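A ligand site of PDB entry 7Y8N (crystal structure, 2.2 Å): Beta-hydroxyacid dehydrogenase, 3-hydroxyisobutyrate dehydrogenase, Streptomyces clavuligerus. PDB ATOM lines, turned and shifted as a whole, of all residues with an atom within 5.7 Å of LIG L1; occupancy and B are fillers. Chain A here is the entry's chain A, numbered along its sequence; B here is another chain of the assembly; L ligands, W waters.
The backbone NH of Thr 36 is in hydrogen-bond range of an oxygen (O16) of LIG L1 (3.0 Å). The side-chain hydroxyl (OG1) of Thr 36 sits at hydrogen-bond distance from an oxygen (O16) of LIG L1, at 2.7 Å. An oxygen (O12) of LIG L1 is in hydrogen-bond range of the backbone carbonyl oxygen of Leu 68, at 2.7 Å. The side-chain amide oxygen (OD1) of Asn 34 lies within hydrogen-bond range of an oxygen (O5) of LIG L1 (2.8 Å). An oxygen (O8) of LIG L1 lies within hydrogen-bond range of the backbone NH (N) of Met 15, 2.8 Å away. The guanidinium group of Arg 234 of chain B lies within salt-bridge range of an oxygen (O2) of LIG L1. The guanidinium group (NE) of Arg 35 lies within salt-bridge range of an oxygen (O16) of LIG L1, 2.9 Å away. The backbone NH (N) of Leu 12 lies within hydrogen-bond range of an oxygen (O5) of LIG L1, at 2.9 Å. The guanidinium group of Arg 39 lies within salt-bridge range of an oxygen (O17) of LIG L1. O12 of LIG L1 is in hydrogen-bond range of O of Thr 69, 3.0 Å away. The side-chain hydroxyl of Thr 69 is in hydrogen-bond range of an oxygen (O1) of LIG L1. The backbone NH (N) of Ser 95 is in hydrogen-bond range of an oxygen (O12) of LIG L1 (3.0 Å). The backbone NH (N) of Gly 13 lies within hydrogen-bond range of an oxygen (O5) of LIG L1, 3.2 Å away. An oxygen (O13) of LIG L1 lies within hydrogen-bond range of the side-chain sulfur of Met 237 of chain B, at 3.6 Å. A nitrogen (N7) of LIG L1 sits at hydrogen-bond distance from the backbone carbonyl oxygen (O) of Ala 232 of chain B, 3.5 Å away.
N of Pro 14 lies close to O8 of LIG L1 (3.5 Å). Gly 11 touches LIG L1. Ser 67 touches LIG L1. Ala 73 touches LIG L1. CG of Leu 77 touches C9 of LIG L1 (3.6 Å). Leu 93 touches LIG L1. CA of Ser 94 touches O12 of LIG L1 (3.6 Å). O of Val 120 touches C20 of LIG L1, at 3.1 Å. Cys 122 touches LIG L1 (O to C19, 3.4 Å). CA of Pro 123 touches O14 of LIG L1 (3.8 Å). CD of Pro 124 touches O14 of LIG L1 (3.4 Å). Tyr 170 touches LIG L1. Hydrophobic or aromatic side chains within 4 Å of LIG L1: Pro 14, Met 15, Leu 68, Ala 73, Leu 77, Pro 124, Tyr 170 and Met 237 of chain B. Within 4 Å of LIG L1: Gly 11, Leu 12, Gly 13, Pro 14, Met 15, Asn 34, Arg 35, Thr 36, Arg 39, Ser 67, Leu 68, Thr 69, Ala 73, Leu 77, Leu 93, Ser 94, Ser 95, Val 120, Cys 122, Pro 123, Pro 124, Tyr 170, Ala 232 of chain B, Arg 234 of chain B and Met 237 of chain B.
Water W10 bridges O14 of LIG L1 (2.6 Å) and O of Ala 232 of chain B (2.9 Å). Water W6 lies within hydrogen-bond range of O9 of LIG L1 (2.7 Å) and N of Arg 234 of chain B (2.9 Å). Water W13 lies within hydrogen-bond range of the side-chain hydroxyl (OH) of Tyr 170 (2.6 Å), an oxygen (O13) of LIG L1 (2.7 Å) and the side-chain hydroxyl (OG) of Ser 241 of chain B (3.0 Å). Water W14 lies within hydrogen-bond range of OG of Ser 67 (2.7 Å), O11 of LIG L1 (2.8 Å) and O of Leu 93 (2.9 Å). Water W12 lies within hydrogen-bond range of N of Arg 35, OD1 of Asn 34 and O6 of LIG L1. Water W4 bridges the guanidinium group (NH1) of Arg 35 and a nitrogen (N2) of LIG L1.
The backbone carbonyl oxygen (O) of Thr 36 lies within hydrogen-bond range of the side-chain amide nitrogen (ND2) of Asn 34, 2.9 Å away. The backbone NH of Leu 68 sits at hydrogen-bond distance from the side-chain hydroxyl of Ser 94 (3.0 Å). OD1 of Asn 34 lies within hydrogen-bond range of N of Leu 12 (2.8 Å). The side-chain hydroxyl of Ser 95 is in hydrogen-bond range of a ring nitrogen (ND1) of His 244 of chain B, at 2.9 Å. The backbone NH of Ala 73 is in hydrogen-bond range of the side-chain carboxylate of Asp 70 (3.3 Å).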
ATOM      1  N   GLY A  11      13.069  -3.301 -18.440  1.00  0.00           N
ATOM      2  CA  GLY A  11      13.854  -4.173 -19.293  1.00  0.00           C
ATOM      3  C   GLY A  11      13.398  -4.090 -20.735  1.00  0.00           C
ATOM      4  O   GLY A  11      12.413  -4.724 -21.125  1.00  0.00           O
ATOM      5  N   LEU A  12      14.125  -3.317 -21.550  1.00  0.00           N
ATOM      6  CA  LEU A  12      13.684  -3.062 -22.916  1.00  0.00           C
ATOM      7  C   LEU A  12      14.647  -3.611 -23.951  1.00  0.00           C
ATOM      8  O   LEU A  12      15.034  -2.917 -24.886  1.00  0.00           O
ATOM      9  CB  LEU A  12      13.472  -1.564 -23.124  1.00  0.00           C
ATOM     10  CG  LEU A  12      12.389  -0.957 -22.228  1.00  0.00           C
ATOM     11  CD1 LEU A  12      12.175   0.511 -22.554  1.00  0.00           C
ATOM     12  CD2 LEU A  12      11.091  -1.736 -22.382  1.00  0.00           C
ATOM     13  N   GLY A  13      15.039  -4.876 -23.785  1.00  0.00           N
ATOM     14  CA  GLY A  13      15.718  -5.593 -24.831  1.00  0.00           C
ATOM     15  C   GLY A  13      14.731  -5.968 -25.933  1.00  0.00           C
ATOM     16  O   GLY A  13      13.605  -5.461 -25.963  1.00  0.00           O
ATOM     17  N   PRO A  14      15.128  -6.862 -26.831  1.00  0.00           N
ATOM     18  CA  PRO A  14      14.235  -7.224 -27.950  1.00  0.00           C
ATOM     19  C   PRO A  14      12.837  -7.658 -27.518  1.00  0.00           C
ATOM     20  O   PRO A  14      11.867  -7.290 -28.183  1.00  0.00           O
ATOM     21  CB  PRO A  14      15.002  -8.370 -28.625  1.00  0.00           C
ATOM     22  CG  PRO A  14      16.432  -8.049 -28.353  1.00  0.00           C
ATOM     23  CD  PRO A  14      16.435  -7.541 -26.938  1.00  0.00           C
ATOM     24  N   MET A  15      12.710  -8.406 -26.422  1.00  0.00           N
ATOM     25  CA  MET A  15      11.386  -8.818 -25.979  1.00  0.00           C
ATOM     26  C   MET A  15      10.651  -7.706 -25.229  1.00  0.00           C
ATOM     27  O   MET A  15       9.430  -7.561 -25.380  1.00  0.00           O
ATOM     28  CB  MET A  15      11.492 -10.066 -25.089  1.00  0.00           C
ATOM     29  CG  MET A  15      12.145 -11.240 -25.798  1.00  0.00           C
ATOM     30  SD  MET A  15      10.940 -12.141 -26.784  1.00  0.00           S
ATOM     31  CE  MET A  15       9.671 -12.452 -25.560  1.00  0.00           C
ATOM     32  N   GLY A  16      11.371  -6.924 -24.421  1.00  0.00           N
ATOM     33  CA  GLY A  16      10.723  -5.828 -23.718  1.00  0.00           C
ATOM     34  C   GLY A  16      10.185  -4.775 -24.662  1.00  0.00           C
ATOM     35  O   GLY A  16       9.103  -4.214 -24.426  1.00  0.00           O
ATOM     36  N   ASN A  34      14.513   1.576 -18.332  1.00  0.00           N
ATOM     37  CA  ASN A  34      15.561   0.712 -18.837  1.00  0.00           C
ATOM     38  C   ASN A  34      16.911   1.257 -18.381  1.00  0.00           C
ATOM     39  O   ASN A  34      17.078   2.474 -18.246  1.00  0.00           O
ATOM     40  CB  ASN A  34      15.519   0.610 -20.363  1.00  0.00           C
ATOM     41  CG  ASN A  34      16.269  -0.608 -20.881  1.00  0.00           C
ATOM     42  OD1 ASN A  34      16.083  -1.719 -20.395  1.00  0.00           O
ATOM     43  ND2 ASN A  34      17.111  -0.387 -21.883  1.00  0.00           N
ATOM     44  N   ARG A  35      17.859   0.350 -18.134  1.00  0.00           N
ATOM     45  CA  ARG A  35      19.215   0.760 -17.786  1.00  0.00           C
ATOM     46  C   ARG A  35      19.792   1.667 -18.872  1.00  0.00           C
ATOM     47  O   ARG A  35      20.312   2.751 -18.585  1.00  0.00           O
ATOM     48  CB  ARG A  35      20.107  -0.464 -17.577  1.00  0.00           C
ATOM     49  CG  ARG A  35      21.587  -0.139 -17.576  1.00  0.00           C
ATOM     50  CD  ARG A  35      22.453  -1.370 -17.325  1.00  0.00           C
ATOM     51  NE  ARG A  35      22.373  -2.330 -18.409  1.00  0.00           N
ATOM     52  CZ  ARG A  35      23.005  -3.506 -18.415  1.00  0.00           C
ATOM     53  NH1 ARG A  35      23.771  -3.872 -17.414  1.00  0.00           N
ATOM     54  NH2 ARG A  35      22.861  -4.311 -19.459  1.00  0.00           N
ATOM     55  N   THR A  36      19.700   1.229 -20.122  1.00  0.00           N
ATOM     56  CA  THR A  36      20.072   2.063 -21.266  1.00  0.00           C
ATOM     57  C   THR A  36      18.826   2.846 -21.677  1.00  0.00           C
ATOM     58  O   THR A  36      17.976   2.337 -22.409  1.00  0.00           O
ATOM     59  CB  THR A  36      20.592   1.204 -22.416  1.00  0.00           C
ATOM     60  OG1 THR A  36      21.650   0.354 -21.930  1.00  0.00           O
ATOM     61  CG2 THR A  36      21.135   2.076 -23.535  1.00  0.00           C
ATOM     62  N   ARG A  39      16.786   3.107 -25.132  1.00  0.00           N
ATOM     63  CA  ARG A  39      15.901   2.090 -25.684  1.00  0.00           C
ATOM     64  C   ARG A  39      14.425   2.352 -25.397  1.00  0.00           C
ATOM     65  O   ARG A  39      13.574   1.628 -25.934  1.00  0.00           O
ATOM     66  CB  ARG A  39      16.313   0.716 -25.164  1.00  0.00           C
ATOM     67  CG  ARG A  39      17.734   0.343 -25.556  1.00  0.00           C
ATOM     68  CD  ARG A  39      18.115  -1.037 -25.070  1.00  0.00           C
ATOM     69  NE  ARG A  39      18.350  -1.947 -26.188  1.00  0.00           N
ATOM     70  CZ  ARG A  39      18.600  -3.244 -26.061  1.00  0.00           C
ATOM     71  NH1 ARG A  39      18.672  -3.817 -24.868  1.00  0.00           N
ATOM     72  NH2 ARG A  39      18.784  -3.978 -27.157  1.00  0.00           N
ATOM     73  N   SER A  67      11.592  -7.988 -17.975  1.00  0.00           N
ATOM     74  CA  SER A  67      12.116  -8.753 -19.104  1.00  0.00           C
ATOM     75  C   SER A  67      13.630  -8.545 -19.118  1.00  0.00           C
ATOM     76  O   SER A  67      14.143  -7.655 -19.809  1.00  0.00           O
ATOM     77  CB  SER A  67      11.464  -8.336 -20.420  1.00  0.00           C
ATOM     78  OG  SER A  67      11.816  -9.219 -21.474  1.00  0.00           O
ATOM     79  N   LEU A  68      14.333  -9.350 -18.340  1.00  0.00           N
ATOM     80  CA  LEU A  68      15.768  -9.196 -18.130  1.00  0.00           C
ATOM     81  C   LEU A  68      16.474 -10.486 -18.511  1.00  0.00           C
ATOM     82  O   LEU A  68      15.841 -11.508 -18.778  1.00  0.00           O
ATOM     83  CB  LEU A  68      16.065  -8.815 -16.674  1.00  0.00           C
ATOM     84  CG  LEU A  68      15.336  -7.560 -16.189  1.00  0.00           C
ATOM     85  CD1 LEU A  68      15.408  -7.451 -14.676  1.00  0.00           C
ATOM     86  CD2 LEU A  68      15.900  -6.309 -16.858  1.00  0.00           C
ATOM     87  N   THR A  69      17.810 -10.432 -18.534  1.00  0.00           N
ATOM     88  CA  THR A  69      18.591 -11.574 -18.989  1.00  0.00           C
ATOM     89  C   THR A  69      18.399 -12.783 -18.079  1.00  0.00           C
ATOM     90  O   THR A  69      18.176 -13.904 -18.551  1.00  0.00           O
ATOM     91  CB  THR A  69      20.081 -11.198 -19.067  1.00  0.00           C
ATOM     92  OG1 THR A  69      20.238 -10.058 -19.915  1.00  0.00           O
ATOM     93  CG2 THR A  69      20.897 -12.350 -19.620  1.00  0.00           C
ATOM     94  N   ASP A  70      18.474 -12.566 -16.766  1.00  0.00           N
ATOM     95  CA  ASP A  70      18.269 -13.635 -15.800  1.00  0.00           C
ATOM     96  C   ASP A  70      17.739 -13.023 -14.514  1.00  0.00           C
ATOM     97  O   ASP A  70      17.402 -11.838 -14.462  1.00  0.00           O
ATOM     98  CB  ASP A  70      19.573 -14.430 -15.596  1.00  0.00           C
ATOM     99  CG  ASP A  70      20.746 -13.539 -15.227  1.00  0.00           C
ATOM    100  OD1 ASP A  70      20.535 -12.349 -14.938  1.00  0.00           O
ATOM    101  OD2 ASP A  70      21.897 -14.041 -15.241  1.00  0.00           O
ATOM    102  N   ALA A  73      19.793 -10.163 -12.584  1.00  0.00           N
ATOM    103  CA  ALA A  73      19.529  -8.803 -13.003  1.00  0.00           C
ATOM    104  C   ALA A  73      18.362  -8.183 -12.249  1.00  0.00           C
ATOM    105  O   ALA A  73      18.299  -6.951 -12.137  1.00  0.00           O
ATOM    106  CB  ALA A  73      19.259  -8.746 -14.510  1.00  0.00           C
ATOM    107  N   ALA A  76      19.849  -6.899  -9.091  1.00  0.00           N
ATOM    108  CA  ALA A  76      20.678  -5.748  -9.417  1.00  0.00           C
ATOM    109  C   ALA A  76      19.841  -4.495  -9.639  1.00  0.00           C
ATOM    110  O   ALA A  76      20.236  -3.393  -9.244  1.00  0.00           O
ATOM    111  CB  ALA A  76      21.522  -6.050 -10.655  1.00  0.00           C
ATOM    112  N   LEU A  77      18.670  -4.643 -10.266  1.00  0.00           N
ATOM    113  CA  LEU A  77      17.843  -3.487 -10.560  1.00  0.00           C
ATOM    114  C   LEU A  77      16.926  -3.120  -9.396  1.00  0.00           C
ATOM    115  O   LEU A  77      16.765  -1.937  -9.085  1.00  0.00           O
ATOM    116  CB  LEU A  77      17.009  -3.735 -11.825  1.00  0.00           C
ATOM    117  CG  LEU A  77      17.672  -3.410 -13.165  1.00  0.00           C
ATOM    118  CD1 LEU A  77      16.656  -3.432 -14.291  1.00  0.00           C
ATOM    119  CD2 LEU A  77      18.383  -2.062 -13.097  1.00  0.00           C
ATOM    120  N   LEU A  93       9.444 -12.151 -16.365  1.00  0.00           N
ATOM    121  CA  LEU A  93       9.458 -12.914 -17.614  1.00  0.00           C
ATOM    122  C   LEU A  93      10.868 -13.255 -18.073  1.00  0.00           C
ATOM    123  O   LEU A  93      11.125 -13.373 -19.275  1.00  0.00           O
ATOM    124  CB  LEU A  93       8.722 -12.141 -18.706  1.00  0.00           C
ATOM    125  CG  LEU A  93       7.277 -11.737 -18.381  1.00  0.00           C
ATOM    126  CD1 LEU A  93       6.643 -11.030 -19.567  1.00  0.00           C
ATOM    127  CD2 LEU A  93       6.458 -12.951 -17.958  1.00  0.00           C
ATOM    128  N   SER A  94      11.804 -13.404 -17.131  1.00  0.00           N
ATOM    129  CA  SER A  94      13.195 -13.689 -17.448  1.00  0.00           C
ATOM    130  C   SER A  94      13.480 -15.171 -17.264  1.00  0.00           C
ATOM    131  O   SER A  94      12.976 -15.805 -16.338  1.00  0.00           O
ATOM    132  CB  SER A  94      14.136 -12.869 -16.557  1.00  0.00           C
ATOM    133  OG  SER A  94      13.654 -11.546 -16.382  1.00  0.00           O
ATOM    134  N   SER A  95      14.295 -15.713 -18.173  1.00  0.00           N
ATOM    135  CA  SER A  95      14.706 -17.105 -18.061  1.00  0.00           C
ATOM    136  C   SER A  95      15.648 -17.303 -16.891  1.00  0.00           C
ATOM    137  O   SER A  95      16.489 -16.450 -16.593  1.00  0.00           O
ATOM    138  CB  SER A  95      15.378 -17.563 -19.349  1.00  0.00           C
ATOM    139  OG  SER A  95      15.897 -18.878 -19.213  1.00  0.00           O
ATOM    140  N   VAL A 120       8.111 -16.964 -21.620  1.00  0.00           N
ATOM    141  CA  VAL A 120       7.517 -16.629 -22.907  1.00  0.00           C
ATOM    142  C   VAL A 120       8.151 -17.499 -23.981  1.00  0.00           C
ATOM    143  O   VAL A 120       9.379 -17.526 -24.128  1.00  0.00           O
ATOM    144  CB  VAL A 120       7.696 -15.141 -23.227  1.00  0.00           C
ATOM    145  CG1 VAL A 120       6.996 -14.799 -24.537  1.00  0.00           C
ATOM    146  CG2 VAL A 120       7.176 -14.282 -22.077  1.00  0.00           C
ATOM    147  N   THR A 121       7.314 -18.225 -24.734  1.00  0.00           N
ATOM    148  CA  THR A 121       7.784 -19.201 -25.702  1.00  0.00           C
ATOM    149  C   THR A 121       7.710 -18.685 -27.145  1.00  0.00           C
ATOM    150  O   THR A 121       7.666 -19.490 -28.072  1.00  0.00           O
ATOM    151  CB  THR A 121       6.981 -20.491 -25.577  1.00  0.00           C
ATOM    152  OG1 THR A 121       5.621 -20.259 -25.976  1.00  0.00           O
ATOM    153  CG2 THR A 121       6.993 -20.985 -24.132  1.00  0.00           C
ATOM    154  N   CYS A 122       7.713 -17.377 -27.343  1.00  0.00           N
ATOM    155  CA  CYS A 122       7.663 -16.786 -28.666  1.00  0.00           C
ATOM    156  C   CYS A 122       8.750 -15.738 -28.810  1.00  0.00           C
ATOM    157  O   CYS A 122       9.210 -15.164 -27.817  1.00  0.00           O
ATOM    158  CB  CYS A 122       6.288 -16.147 -28.920  1.00  0.00           C
ATOM    159  SG  CYS A 122       5.973 -14.628 -28.001  1.00  0.00           S
ATOM    160  N   PRO A 123       9.206 -15.480 -30.037  1.00  0.00           N
ATOM    161  CA  PRO A 123      10.170 -14.399 -30.266  1.00  0.00           C
ATOM    162  C   PRO A 123       9.503 -13.049 -30.142  1.00  0.00           C
ATOM    163  O   PRO A 123       8.267 -12.975 -29.988  1.00  0.00           O
ATOM    164  CB  PRO A 123      10.653 -14.672 -31.697  1.00  0.00           C
ATOM    165  CG  PRO A 123       9.479 -15.306 -32.349  1.00  0.00           C
ATOM    166  CD  PRO A 123       8.887 -16.195 -31.285  1.00  0.00           C
ATOM    167  N   PRO A 124      10.261 -11.947 -30.202  1.00  0.00           N
ATOM    168  CA  PRO A 124       9.637 -10.616 -30.105  1.00  0.00           C
ATOM    169  C   PRO A 124       8.522 -10.371 -31.111  1.00  0.00           C
ATOM    170  O   PRO A 124       7.512  -9.757 -30.776  1.00  0.00           O
ATOM    171  CB  PRO A 124      10.821  -9.666 -30.326  1.00  0.00           C
ATOM    172  CG  PRO A 124      11.996 -10.430 -29.837  1.00  0.00           C
ATOM    173  CD  PRO A 124      11.738 -11.841 -30.254  1.00  0.00           C
ATOM    174  N   TYR A 170       9.632 -23.881 -19.319  1.00  0.00           N
ATOM    175  CA  TYR A 170      10.384 -23.122 -20.304  1.00  0.00           C
ATOM    176  C   TYR A 170      11.653 -23.857 -20.718  1.00  0.00           C
ATOM    177  O   TYR A 170      11.948 -23.999 -21.913  1.00  0.00           O
ATOM    178  CB  TYR A 170      10.724 -21.736 -19.765  1.00  0.00           C
ATOM    179  CG  TYR A 170      11.391 -20.853 -20.787  1.00  0.00           C
ATOM    180  CD1 TYR A 170      10.661 -20.246 -21.793  1.00  0.00           C
ATOM    181  CD2 TYR A 170      12.764 -20.627 -20.743  1.00  0.00           C
ATOM    182  CE1 TYR A 170      11.277 -19.436 -22.738  1.00  0.00           C
ATOM    183  CE2 TYR A 170      13.379 -19.820 -21.671  1.00  0.00           C
ATOM    184  CZ  TYR A 170      12.636 -19.225 -22.668  1.00  0.00           C
ATOM    185  OH  TYR A 170      13.245 -18.431 -23.599  1.00  0.00           O
ATOM    186  N   ALA B 232      17.031  -9.127 -32.787  1.00  0.00           N
ATOM    187  CA  ALA B 232      16.100 -10.110 -32.268  1.00  0.00           C
ATOM    188  C   ALA B 232      16.646 -10.899 -31.081  1.00  0.00           C
ATOM    189  O   ALA B 232      15.853 -11.377 -30.268  1.00  0.00           O
ATOM    190  CB  ALA B 232      15.696 -11.097 -33.374  1.00  0.00           C
ATOM    191  N   ASP B 233      17.967 -11.014 -30.962  1.00  0.00           N
ATOM    192  CA  ASP B 233      18.562 -11.791 -29.892  1.00  0.00           C
ATOM    193  C   ASP B 233      20.033 -11.418 -29.767  1.00  0.00           C
ATOM    194  O   ASP B 233      20.706 -11.171 -30.771  1.00  0.00           O
ATOM    195  CB  ASP B 233      18.417 -13.295 -30.135  1.00  0.00           C
ATOM    196  CG  ASP B 233      19.344 -13.795 -31.230  1.00  0.00           C
ATOM    197  OD1 ASP B 233      19.014 -13.616 -32.425  1.00  0.00           O
ATOM    198  OD2 ASP B 233      20.404 -14.369 -30.900  1.00  0.00           O
ATOM    199  N   ARG B 234      20.526 -11.383 -28.526  1.00  0.00           N
ATOM    200  CA  ARG B 234      21.960 -11.261 -28.268  1.00  0.00           C
ATOM    201  C   ARG B 234      22.519 -12.623 -27.894  1.00  0.00           C
ATOM    202  O   ARG B 234      21.881 -13.390 -27.162  1.00  0.00           O
ATOM    203  CB  ARG B 234      22.229 -10.267 -27.134  1.00  0.00           C
ATOM    204  CG  ARG B 234      22.144  -8.806 -27.547  1.00  0.00           C
ATOM    205  CD  ARG B 234      22.155  -7.883 -26.341  1.00  0.00           C
ATOM    206  NE  ARG B 234      23.369  -8.023 -25.549  1.00  0.00           N
ATOM    207  CZ  ARG B 234      23.425  -8.591 -24.351  1.00  0.00           C
ATOM    208  NH1 ARG B 234      22.340  -9.082 -23.771  1.00  0.00           N
ATOM    209  NH2 ARG B 234      24.593  -8.657 -23.723  1.00  0.00           N
ATOM    210  N   MET B 237      22.707 -13.229 -24.219  1.00  0.00           N
ATOM    211  CA  MET B 237      21.438 -13.676 -23.664  1.00  0.00           C
ATOM    212  C   MET B 237      21.240 -15.168 -23.904  1.00  0.00           C
ATOM    213  O   MET B 237      20.708 -15.884 -23.047  1.00  0.00           O
ATOM    214  CB  MET B 237      20.291 -12.863 -24.253  1.00  0.00           C
ATOM    215  CG  MET B 237      18.896 -13.288 -23.802  1.00  0.00           C
ATOM    216  SD  MET B 237      18.165 -14.635 -24.760  1.00  0.00           S
ATOM    217  CE  MET B 237      18.262 -13.964 -26.418  1.00  0.00           C
ATOM    218  N   SER B 241      20.775 -18.417 -21.390  1.00  0.00           N
ATOM    219  CA  SER B 241      19.646 -19.330 -21.575  1.00  0.00           C
ATOM    220  C   SER B 241      20.099 -20.782 -21.551  1.00  0.00           C
ATOM    221  O   SER B 241      19.476 -21.623 -20.900  1.00  0.00           O
ATOM    222  CB  SER B 241      18.935 -19.007 -22.883  1.00  0.00           C
ATOM    223  OG  SER B 241      17.944 -19.983 -23.170  1.00  0.00           O
ATOM    224  N   HIS B 244      21.115 -21.823 -18.184  1.00  0.00           N
ATOM    225  CA  HIS B 244      19.932 -22.144 -17.382  1.00  0.00           C
ATOM    226  C   HIS B 244      19.489 -23.579 -17.634  1.00  0.00           C
ATOM    227  O   HIS B 244      19.117 -24.288 -16.694  1.00  0.00           O
ATOM    228  CB  HIS B 244      18.800 -21.164 -17.684  1.00  0.00           C
ATOM    229  CG  HIS B 244      19.156 -19.737 -17.419  1.00  0.00           C
ATOM    230  ND1 HIS B 244      18.551 -18.686 -18.071  1.00  0.00           N
ATOM    231  CD2 HIS B 244      20.059 -19.193 -16.576  1.00  0.00           C
ATOM    232  CE1 HIS B 244      19.072 -17.547 -17.633  1.00  0.00           C
ATOM    233  NE2 HIS B 244      19.981 -17.826 -16.726  1.00  0.00           N
HETATM  234  P1  LIG L   1      18.361  -9.337 -23.168  1.00  0.00           P
HETATM  235  O1  LIG L   1      18.328 -10.459 -22.186  1.00  0.00           O
HETATM  236  O2  LIG L   1      19.475  -9.272 -24.136  1.00  0.00           O
HETATM  237  O3  LIG L   1      18.266  -7.960 -22.378  1.00  0.00           O
HETATM  238  C1  LIG L   1      17.023  -7.736 -21.690  1.00  0.00           C
HETATM  239  C2  LIG L   1      17.168  -6.545 -20.767  1.00  0.00           C
HETATM  240  O4  LIG L   1      17.961  -6.926 -19.625  1.00  0.00           O
HETATM  241  C3  LIG L   1      17.827  -5.287 -21.343  1.00  0.00           C
HETATM  242  O5  LIG L   1      16.882  -4.234 -21.284  1.00  0.00           O
HETATM  243  C4  LIG L   1      19.073  -5.076 -20.480  1.00  0.00           C
HETATM  244  O6  LIG L   1      19.335  -3.712 -20.147  1.00  0.00           O
HETATM  245  C5  LIG L   1      18.642  -5.784 -19.204  1.00  0.00           C
HETATM  246  N1  LIG L   1      19.726  -6.183 -18.327  1.00  0.00           N
HETATM  247  C6  LIG L   1      20.512  -7.299 -18.425  1.00  0.00           C
HETATM  248  N2  LIG L   1      21.374  -7.411 -17.455  1.00  0.00           N
HETATM  249  C7  LIG L   1      21.145  -6.308 -16.652  1.00  0.00           C
HETATM  250  C8  LIG L   1      21.741  -5.856 -15.463  1.00  0.00           C
HETATM  251  N3  LIG L   1      22.721  -6.497 -14.835  1.00  0.00           N
HETATM  252  N4  LIG L   1      21.260  -4.713 -14.922  1.00  0.00           N
HETATM  253  C9  LIG L   1      20.273  -4.068 -15.556  1.00  0.00           C
HETATM  254  N5  LIG L   1      19.635  -4.404 -16.673  1.00  0.00           N
HETATM  255  C10 LIG L   1      20.127  -5.540 -17.188  1.00  0.00           C
HETATM  256  O7  LIG L   1      16.989  -9.280 -23.979  1.00  0.00           O
HETATM  257  P2  LIG L   1      15.840 -10.270 -24.472  1.00  0.00           P
HETATM  258  O8  LIG L   1      14.615  -9.444 -24.598  1.00  0.00           O
HETATM  259  O9  LIG L   1      16.278 -11.018 -25.673  1.00  0.00           O
HETATM  260  O10 LIG L   1      15.692 -11.274 -23.249  1.00  0.00           O
HETATM  261  C11 LIG L   1      14.685 -11.090 -22.229  1.00  0.00           C
HETATM  262  C12 LIG L   1      14.424 -12.396 -21.548  1.00  0.00           C
HETATM  263  O11 LIG L   1      13.422 -13.129 -22.297  1.00  0.00           O
HETATM  264  C13 LIG L   1      15.627 -13.343 -21.391  1.00  0.00           C
HETATM  265  O12 LIG L   1      15.653 -13.898 -20.083  1.00  0.00           O
HETATM  266  C14 LIG L   1      15.381 -14.385 -22.483  1.00  0.00           C
HETATM  267  O13 LIG L   1      15.928 -15.651 -22.184  1.00  0.00           O
HETATM  268  C15 LIG L   1      13.867 -14.431 -22.549  1.00  0.00           C
HETATM  269  N6  LIG L   1      13.367 -14.803 -23.897  1.00  0.00           N
HETATM  270  C16 LIG L   1      14.022 -14.424 -25.030  1.00  0.00           C
HETATM  271  C17 LIG L   1      13.444 -14.575 -26.263  1.00  0.00           C
HETATM  272  C18 LIG L   1      13.998 -13.900 -27.454  1.00  0.00           C
HETATM  273  O14 LIG L   1      13.527 -14.211 -28.548  1.00  0.00           O
HETATM  274  N7  LIG L   1      14.917 -12.962 -27.340  1.00  0.00           N
HETATM  275  C19 LIG L   1      12.238 -15.428 -26.371  1.00  0.00           C
HETATM  276  C20 LIG L   1      11.556 -15.599 -25.109  1.00  0.00           C
HETATM  277  C21 LIG L   1      12.221 -15.534 -23.997  1.00  0.00           C
HETATM  278  P3  LIG L   1      20.046  -2.829 -21.287  1.00  0.00           P
HETATM  279  O15 LIG L   1      21.176  -3.583 -21.884  1.00  0.00           O
HETATM  280  O16 LIG L   1      20.516  -1.637 -20.524  1.00  0.00           O
HETATM  281  O17 LIG L   1      19.014  -2.452 -22.304  1.00  0.00           O
HETATM  282  C1  LG2 L   2      12.146 -17.981 -29.468  1.00  0.00           C
HETATM  283  C2  LG2 L   2      11.547 -19.355 -29.269  1.00  0.00           C
HETATM  284  C3  LG2 L   2      13.079 -17.905 -28.378  1.00  0.00           C
HETATM  285  C4  LG2 L   2      11.322 -19.298 -27.744  1.00  0.00           C
HETATM  286  C5  LG2 L   2      14.504 -17.426 -28.464  1.00  0.00           C
HETATM  287  C6  LG2 L   2      15.029 -16.949 -29.649  1.00  0.00           C
HETATM  288  C7  LG2 L   2      15.237 -17.464 -27.315  1.00  0.00           C
HETATM  289  C8  LG2 L   2      16.529 -17.041 -27.366  1.00  0.00           C
HETATM  290  C9  LG2 L   2      16.335 -16.525 -29.698  1.00  0.00           C
HETATM  291  C10 LG2 L   2      17.075 -16.567 -28.542  1.00  0.00           C
HETATM  292  F1  LG2 L   2      14.293 -16.908 -30.775  1.00  0.00           F
HETATM  293  F2  LG2 L   2      17.268 -17.100 -26.237  1.00  0.00           F
HETATM  294  N1  LG2 L   2      12.466 -18.645 -27.210  1.00  0.00           N
HETATM  295  O   HOH W   1      18.445 -15.511 -20.982  1.00  0.00           O
HETATM  296  O   HOH W   2      13.749  -7.401 -23.104  1.00  0.00           O
HETATM  297  O   HOH W   3      19.561  -6.517 -25.083  1.00  0.00           O
HETATM  298  O   HOH W   4      24.690  -6.465 -18.026  1.00  0.00           O
HETATM  299  O   HOH W   5      22.015  -3.340 -12.717  1.00  0.00           O
HETATM  300  O   HOH W   6      18.735 -10.410 -26.508  1.00  0.00           O
HETATM  301  O   HOH W   7      21.815  -5.702 -23.262  1.00  0.00           O
HETATM  302  O   HOH W   8      24.374  -5.762 -12.369  1.00  0.00           O
HETATM  303  O   HOH W   9      23.045  -9.708 -17.391  1.00  0.00           O
HETATM  304  O   HOH W  10      14.403 -13.781 -30.966  1.00  0.00           O
HETATM  305  O   HOH W  11      10.666 -15.704 -21.059  1.00  0.00           O
HETATM  306  O   HOH W  12      17.420  -2.443 -17.913  1.00  0.00           O
HETATM  307  O   HOH W  13      15.774 -17.938 -23.645  1.00  0.00           O
HETATM  308  O   HOH W  14      11.072 -11.811 -21.684  1.00  0.00           O
